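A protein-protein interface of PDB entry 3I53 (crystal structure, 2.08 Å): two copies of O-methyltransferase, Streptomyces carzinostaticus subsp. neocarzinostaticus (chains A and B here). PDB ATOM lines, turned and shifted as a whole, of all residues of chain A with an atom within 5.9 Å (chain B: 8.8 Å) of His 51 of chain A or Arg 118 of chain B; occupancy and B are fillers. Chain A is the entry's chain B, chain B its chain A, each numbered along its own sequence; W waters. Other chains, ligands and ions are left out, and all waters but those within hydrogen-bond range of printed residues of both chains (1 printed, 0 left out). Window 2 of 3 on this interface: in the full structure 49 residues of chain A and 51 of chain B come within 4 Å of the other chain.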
ATOM      1  N   THR A  27      23.196  27.580  12.243  1.00  0.00           N
ATOM      2  CA  THR A  27      24.070  27.017  11.221  1.00  0.00           C
ATOM      3  C   THR A  27      23.834  27.680   9.859  1.00  0.00           C
ATOM      4  O   THR A  27      24.787  28.007   9.142  1.00  0.00           O
ATOM      5  CB  THR A  27      23.837  25.506  11.089  1.00  0.00           C
ATOM      6  OG1 THR A  27      23.922  24.899  12.381  1.00  0.00           O
ATOM      7  CG2 THR A  27      24.888  24.878  10.176  1.00  0.00           C
ATOM      8  N   LEU A  28      22.563  27.865   9.503  1.00  0.00           N
ATOM      9  CA  LEU A  28      22.228  28.507   8.236  1.00  0.00           C
ATOM     10  C   LEU A  28      22.393  30.022   8.364  1.00  0.00           C
ATOM     11  O   LEU A  28      22.256  30.751   7.382  1.00  0.00           O
ATOM     12  CB  LEU A  28      20.788  28.175   7.819  1.00  0.00           C
ATOM     13  CG  LEU A  28      20.486  26.728   7.421  1.00  0.00           C
ATOM     14  CD1 LEU A  28      19.019  26.603   7.051  1.00  0.00           C
ATOM     15  CD2 LEU A  28      21.359  26.309   6.249  1.00  0.00           C
ATOM     16  N   ALA A  45      16.410  31.376   2.100  1.00  0.00           N
ATOM     17  CA  ALA A  45      16.776  30.072   1.564  1.00  0.00           C
ATOM     18  C   ALA A  45      17.759  30.220   0.407  1.00  0.00           C
ATOM     19  O   ALA A  45      18.597  29.346   0.172  1.00  0.00           O
ATOM     20  CB  ALA A  45      15.526  29.327   1.096  1.00  0.00           C
ATOM     21  N   ALA A  48      21.066  31.249   2.183  1.00  0.00           N
ATOM     22  CA  ALA A  48      21.562  30.131   2.981  1.00  0.00           C
ATOM     23  C   ALA A  48      21.613  28.803   2.232  1.00  0.00           C
ATOM     24  O   ALA A  48      22.027  27.780   2.795  1.00  0.00           O
ATOM     25  CB  ALA A  48      20.717  29.980   4.241  1.00  0.00           C
ATOM     26  N   GLY A  49      21.201  28.809   0.969  1.00  0.00           N
ATOM     27  CA  GLY A  49      21.214  27.579   0.198  1.00  0.00           C
ATOM     28  C   GLY A  49      20.319  26.492   0.775  1.00  0.00           C
ATOM     29  O   GLY A  49      20.734  25.340   0.903  1.00  0.00           O
ATOM     30  N   ALA A  50      19.086  26.849   1.120  1.00  0.00           N
ATOM     31  CA  ALA A  50      18.144  25.888   1.681  1.00  0.00           C
ATOM     32  C   ALA A  50      16.922  25.705   0.785  1.00  0.00           C
ATOM     33  O   ALA A  50      16.846  26.273  -0.298  1.00  0.00           O
ATOM     34  CB  ALA A  50      17.707  26.341   3.066  1.00  0.00           C
ATOM     35  N   HIS A  51      15.981  24.884   1.242  1.00  0.00           N
ATOM     36  CA  HIS A  51      14.734  24.627   0.525  1.00  0.00           C
ATOM     37  C   HIS A  51      13.735  25.637   1.108  1.00  0.00           C
ATOM     38  O   HIS A  51      13.405  25.558   2.290  1.00  0.00           O
ATOM     39  CB  HIS A  51      14.277  23.191   0.802  1.00  0.00           C
ATOM     40  CG  HIS A  51      13.019  22.799   0.089  1.00  0.00           C
ATOM     41  ND1 HIS A  51      12.944  22.688  -1.284  1.00  0.00           N
ATOM     42  CD2 HIS A  51      11.799  22.442   0.564  1.00  0.00           C
ATOM     43  CE1 HIS A  51      11.735  22.272  -1.623  1.00  0.00           C
ATOM     44  NE2 HIS A  51      11.022  22.115  -0.521  1.00  0.00           N
ATOM     45  N   ALA A  52      13.265  26.579   0.289  1.00  0.00           N
ATOM     46  CA  ALA A  52      12.351  27.631   0.751  1.00  0.00           C
ATOM     47  C   ALA A  52      11.127  27.181   1.547  1.00  0.00           C
ATOM     48  O   ALA A  52      10.873  27.705   2.634  1.00  0.00           O
ATOM     49  CB  ALA A  52      11.913  28.507  -0.426  1.00  0.00           C
ATOM     50  N   ASP A  53      10.360  26.230   1.026  1.00  0.00           N
ATOM     51  CA  ASP A  53       9.183  25.771   1.762  1.00  0.00           C
ATOM     52  C   ASP A  53       9.574  25.233   3.131  1.00  0.00           C
ATOM     53  O   ASP A  53       8.959  25.588   4.145  1.00  0.00           O
ATOM     54  CB  ASP A  53       8.426  24.682   0.996  1.00  0.00           C
ATOM     55  CG  ASP A  53       7.274  24.100   1.808  1.00  0.00           C
ATOM     56  OD1 ASP A  53       6.421  24.893   2.279  1.00  0.00           O
ATOM     57  OD2 ASP A  53       7.214  22.855   1.984  1.00  0.00           O
ATOM     58  N   SER A  54      10.592  24.375   3.163  1.00  0.00           N
ATOM     59  CA  SER A  54      11.040  23.805   4.430  1.00  0.00           C
ATOM     60  C   SER A  54      11.614  24.873   5.359  1.00  0.00           C
ATOM     61  O   SER A  54      11.382  24.825   6.563  1.00  0.00           O
ATOM     62  CB  SER A  54      12.084  22.709   4.200  1.00  0.00           C
ATOM     63  OG  SER A  54      11.539  21.652   3.425  1.00  0.00           O
ATOM     64  N   LEU A  55      12.347  25.838   4.810  1.00  0.00           N
ATOM     65  CA  LEU A  55      12.927  26.883   5.649  1.00  0.00           C
ATOM     66  C   LEU A  55      11.825  27.721   6.304  1.00  0.00           C
ATOM     67  O   LEU A  55      11.935  28.142   7.459  1.00  0.00           O
ATOM     68  CB  LEU A  55      13.850  27.794   4.829  1.00  0.00           C
ATOM     69  CG  LEU A  55      14.472  28.956   5.619  1.00  0.00           C
ATOM     70  CD1 LEU A  55      15.558  28.439   6.555  1.00  0.00           C
ATOM     71  CD2 LEU A  55      15.061  29.970   4.651  1.00  0.00           C
ATOM     72  N   ASP A  56      10.753  27.951   5.559  1.00  0.00           N
ATOM     73  CA  ASP A  56       9.638  28.731   6.070  1.00  0.00           C
ATOM     74  C   ASP A  56       8.967  28.020   7.246  1.00  0.00           C
ATOM     75  O   ASP A  56       8.502  28.656   8.197  1.00  0.00           O
ATOM     76  CB  ASP A  56       8.626  28.981   4.951  1.00  0.00           C
ATOM     77  CG  ASP A  56       7.429  29.766   5.424  1.00  0.00           C
ATOM     78  OD1 ASP A  56       7.626  30.796   6.103  1.00  0.00           O
ATOM     79  OD2 ASP A  56       6.293  29.350   5.119  1.00  0.00           O
ATOM     80  N   ASN A 100      28.791  23.879  12.475  1.00  0.00           N
ATOM     81  CA  ASN A 100      30.123  23.991  11.898  1.00  0.00           C
ATOM     82  C   ASN A 100      31.106  24.313  13.020  1.00  0.00           C
ATOM     83  O   ASN A 100      32.297  24.045  12.897  1.00  0.00           O
ATOM     84  CB  ASN A 100      30.160  25.091  10.837  1.00  0.00           C
ATOM     85  CG  ASN A 100      29.493  24.669   9.548  1.00  0.00           C
ATOM     86  OD1 ASN A 100      29.918  23.709   8.904  1.00  0.00           O
ATOM     87  ND2 ASN A 100      28.440  25.382   9.162  1.00  0.00           N
ATOM     88  N   GLU B 112      19.027  15.136  12.520  1.00  0.00           N
ATOM     89  CA  GLU B 112      19.371  15.361  11.114  1.00  0.00           C
ATOM     90  C   GLU B 112      18.462  16.405  10.446  1.00  0.00           C
ATOM     91  O   GLU B 112      18.343  16.432   9.225  1.00  0.00           O
ATOM     92  CB  GLU B 112      19.274  14.043  10.319  1.00  0.00           C
ATOM     93  CG  GLU B 112      20.001  12.822  10.910  1.00  0.00           C
ATOM     94  CD  GLU B 112      21.528  12.950  10.971  1.00  0.00           C
ATOM     95  OE1 GLU B 112      22.098  13.872  10.342  1.00  0.00           O
ATOM     96  OE2 GLU B 112      22.165  12.105  11.649  1.00  0.00           O
ATOM     97  N   LEU B 113      17.831  17.255  11.251  1.00  0.00           N
ATOM     98  CA  LEU B 113      16.911  18.283  10.757  1.00  0.00           C
ATOM     99  C   LEU B 113      17.483  19.200   9.668  1.00  0.00           C
ATOM    100  O   LEU B 113      16.749  19.679   8.804  1.00  0.00           O
ATOM    101  CB  LEU B 113      16.423  19.139  11.928  1.00  0.00           C
ATOM    102  CG  LEU B 113      15.434  20.277  11.620  1.00  0.00           C
ATOM    103  CD1 LEU B 113      14.141  19.715  11.055  1.00  0.00           C
ATOM    104  CD2 LEU B 113      15.162  21.054  12.893  1.00  0.00           C
ATOM    105  N   ALA B 114      18.790  19.440   9.708  1.00  0.00           N
ATOM    106  CA  ALA B 114      19.402  20.316   8.719  1.00  0.00           C
ATOM    107  C   ALA B 114      19.209  19.755   7.316  1.00  0.00           C
ATOM    108  O   ALA B 114      19.110  20.500   6.340  1.00  0.00           O
ATOM    109  CB  ALA B 114      20.875  20.497   9.011  1.00  0.00           C
ATOM    110  N   HIS B 115      19.161  18.436   7.210  1.00  0.00           N
ATOM    111  CA  HIS B 115      18.972  17.840   5.911  1.00  0.00           C
ATOM    112  C   HIS B 115      17.586  18.152   5.364  1.00  0.00           C
ATOM    113  O   HIS B 115      17.429  18.478   4.187  1.00  0.00           O
ATOM    114  CB  HIS B 115      19.162  16.332   5.979  1.00  0.00           C
ATOM    115  CG  HIS B 115      18.873  15.642   4.685  1.00  0.00           C
ATOM    116  ND1 HIS B 115      17.730  14.905   4.474  1.00  0.00           N
ATOM    117  CD2 HIS B 115      19.569  15.596   3.528  1.00  0.00           C
ATOM    118  CE1 HIS B 115      17.732  14.430   3.242  1.00  0.00           C
ATOM    119  NE2 HIS B 115      18.840  14.836   2.648  1.00  0.00           N
ATOM    120  N   SER B 116      16.581  18.047   6.226  1.00  0.00           N
ATOM    121  CA  SER B 116      15.205  18.319   5.830  1.00  0.00           C
ATOM    122  C   SER B 116      15.031  19.786   5.487  1.00  0.00           C
ATOM    123  O   SER B 116      14.278  20.126   4.586  1.00  0.00           O
ATOM    124  CB  SER B 116      14.228  17.932   6.952  1.00  0.00           C
ATOM    125  OG  SER B 116      14.152  16.522   7.111  1.00  0.00           O
ATOM    126  N   ILE B 117      15.724  20.664   6.200  1.00  0.00           N
ATOM    127  CA  ILE B 117      15.589  22.086   5.912  1.00  0.00           C
ATOM    128  C   ILE B 117      16.246  22.432   4.575  1.00  0.00           C
ATOM    129  O   ILE B 117      15.759  23.287   3.835  1.00  0.00           O
ATOM    130  CB  ILE B 117      16.201  22.953   7.048  1.00  0.00           C
ATOM    131  CG1 ILE B 117      15.446  22.700   8.369  1.00  0.00           C
ATOM    132  CG2 ILE B 117      16.165  24.429   6.671  1.00  0.00           C
ATOM    133  CD1 ILE B 117      13.928  22.783   8.269  1.00  0.00           C
ATOM    134  N   ARG B 118      17.343  21.747   4.253  1.00  0.00           N
ATOM    135  CA  ARG B 118      18.046  21.992   3.004  1.00  0.00           C
ATOM    136  C   ARG B 118      17.429  21.276   1.799  1.00  0.00           C
ATOM    137  O   ARG B 118      17.583  21.729   0.657  1.00  0.00           O
ATOM    138  CB  ARG B 118      19.513  21.567   3.138  1.00  0.00           C
ATOM    139  CG  ARG B 118      20.376  22.535   3.950  1.00  0.00           C
ATOM    140  CD  ARG B 118      21.742  21.933   4.281  1.00  0.00           C
ATOM    141  NE  ARG B 118      22.623  22.897   4.935  1.00  0.00           N
ATOM    142  CZ  ARG B 118      23.453  22.600   5.933  1.00  0.00           C
ATOM    143  NH1 ARG B 118      23.518  21.359   6.404  1.00  0.00           N
ATOM    144  NH2 ARG B 118      24.221  23.550   6.463  1.00  0.00           N
ATOM    145  N   THR B 119      16.717  20.178   2.037  1.00  0.00           N
ATOM    146  CA  THR B 119      16.154  19.421   0.919  1.00  0.00           C
ATOM    147  C   THR B 119      14.650  19.208   0.906  1.00  0.00           C
ATOM    148  O   THR B 119      14.094  18.850  -0.135  1.00  0.00           O
ATOM    149  CB  THR B 119      16.793  18.012   0.815  1.00  0.00           C
ATOM    150  OG1 THR B 119      16.287  17.180   1.866  1.00  0.00           O
ATOM    151  CG2 THR B 119      18.324  18.093   0.916  1.00  0.00           C
ATOM    152  N   GLY B 120      13.989  19.412   2.043  1.00  0.00           N
ATOM    153  CA  GLY B 120      12.557  19.179   2.094  1.00  0.00           C
ATOM    154  C   GLY B 120      12.256  17.694   2.214  1.00  0.00           C
ATOM    155  O   GLY B 120      11.101  17.282   2.252  1.00  0.00           O
ATOM    156  N   GLN B 121      13.305  16.880   2.264  1.00  0.00           N
ATOM    157  CA  GLN B 121      13.160  15.431   2.387  1.00  0.00           C
ATOM    158  C   GLN B 121      13.215  15.017   3.861  1.00  0.00           C
ATOM    159  O   GLN B 121      13.744  15.749   4.694  1.00  0.00           O
ATOM    160  CB  GLN B 121      14.265  14.724   1.593  1.00  0.00           C
ATOM    161  CG  GLN B 121      13.983  14.647   0.098  1.00  0.00           C
ATOM    162  CD  GLN B 121      12.613  14.045  -0.194  1.00  0.00           C
ATOM    163  OE1 GLN B 121      11.621  14.762  -0.343  1.00  0.00           O
ATOM    164  NE2 GLN B 121      12.548  12.715  -0.251  1.00  0.00           N
ATOM    165  N   LEU B 291       7.633  16.626   9.018  1.00  0.00           N
ATOM    166  CA  LEU B 291       8.692  16.855   8.050  1.00  0.00           C
ATOM    167  C   LEU B 291       9.898  15.922   8.278  1.00  0.00           C
ATOM    168  O   LEU B 291      10.401  15.312   7.335  1.00  0.00           O
ATOM    169  CB  LEU B 291       9.167  18.312   8.101  1.00  0.00           C
ATOM    170  CG  LEU B 291      10.423  18.622   7.285  1.00  0.00           C
ATOM    171  CD1 LEU B 291      10.203  18.331   5.779  1.00  0.00           C
ATOM    172  CD2 LEU B 291      10.792  20.072   7.520  1.00  0.00           C
ATOM    173  N   GLY B 295       8.583  13.730   5.718  1.00  0.00           N
ATOM    174  CA  GLY B 295       8.589  14.761   4.700  1.00  0.00           C
ATOM    175  C   GLY B 295       7.129  15.169   4.544  1.00  0.00           C
ATOM    176  O   GLY B 295       6.739  15.788   3.561  1.00  0.00           O
HETATM  177  O   HOH W   1      27.306  24.534   6.502  1.00  0.00           O
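O of Ser 116 of chain B lies within hydrogen-bond range of OG of Ser 54 of chain A, 3.3 Å away.
N of His 51 of chain A lies within hydrogen-bond range of O of Ile 117 of chain B (3.1 Å).
The side-chain hydroxyl (OG) of Ser 116 of chain B sits at hydrogen-bond distance from the backbone carbonyl oxygen (O) of Gln 121 of chain B (2.6 Å).
N of Ala 50 of chain A is in hydrogen-bond range of O of Ala 45 of chain A, 2.7 Å away.
Thr 27 of chain A touches Arg 118 of chain B (CG2 to NH2, 3.999 Å).
CG2 of Ile 117 of chain B touches CD1 of Leu 28 of chain A, at 3.6 Å.
Arg 118 of chain B touches Leu 28 of chain A (NE to CD2, 3.9 Å).
CB of Ala 50 of chain A touches O of Ile 117 of chain B (3.7 Å).
Arg 118 of chain B touches His 51 of chain A.
CA of Gly 120 of chain B touches CD2 of His 51 of chain A (3.7 Å).
Ile 117 of chain B touches Ser 54 of chain A.
OG of Ser 54 of chain A touches CA of Gly 120 of chain B, 3.0 Å away.
Printed residues of chain B within 4 Å of Leu 28 of chain A: Ile 117 and Arg 118.
Of chain B, only Ile 117 (3.7 Å) comes within 4 Å of Ala 50 of chain A.
Of the printed residues of chain B, His 51 of chain A touches Ile 117, Arg 118 and Gly 120.
Ala 52 of chain A touches none of the printed residues of chain B.
Asp 56 of chain A touches none of the printed residues of chain B.
Printed residues of chain A within 4 Å of Ser 116 of chain B: Ser 54.
Of the printed residues of chain A, Arg 118 of chain B touches Thr 27, Leu 28 and His 51.
Of the printed residues of chain A, Gly 120 of chain B touches His 51 (3.7 Å) and Ser 54 (3.0 Å).
The nearest printed residue of chain B that does not touch His 51 of chain A is Thr 119 of chain B (4.002 Å).
The nearest printed residue of chain B that does not touch Ser 54 of chain A is Leu 291 of chain B (4.3 Å).
Of the 13 printed residues of chain A, 5 touch a printed residue of chain B.
Of the 12 printed residues of chain B, 4 touch a printed residue of chain A.
Hydrophobic or aromatic side chains of chain B that line the printed part of chain A: Ile 117.
Among the printed residues, 10 pairs touch across the chains.
No position is printed for both chains.
Water W1 lies within hydrogen-bond range of the side-chain amide nitrogen (ND2) of Asn 100 of chain A (3.0 Å) and the guanidinium group (NH2) of Arg 118 of chain B (3.2 Å).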
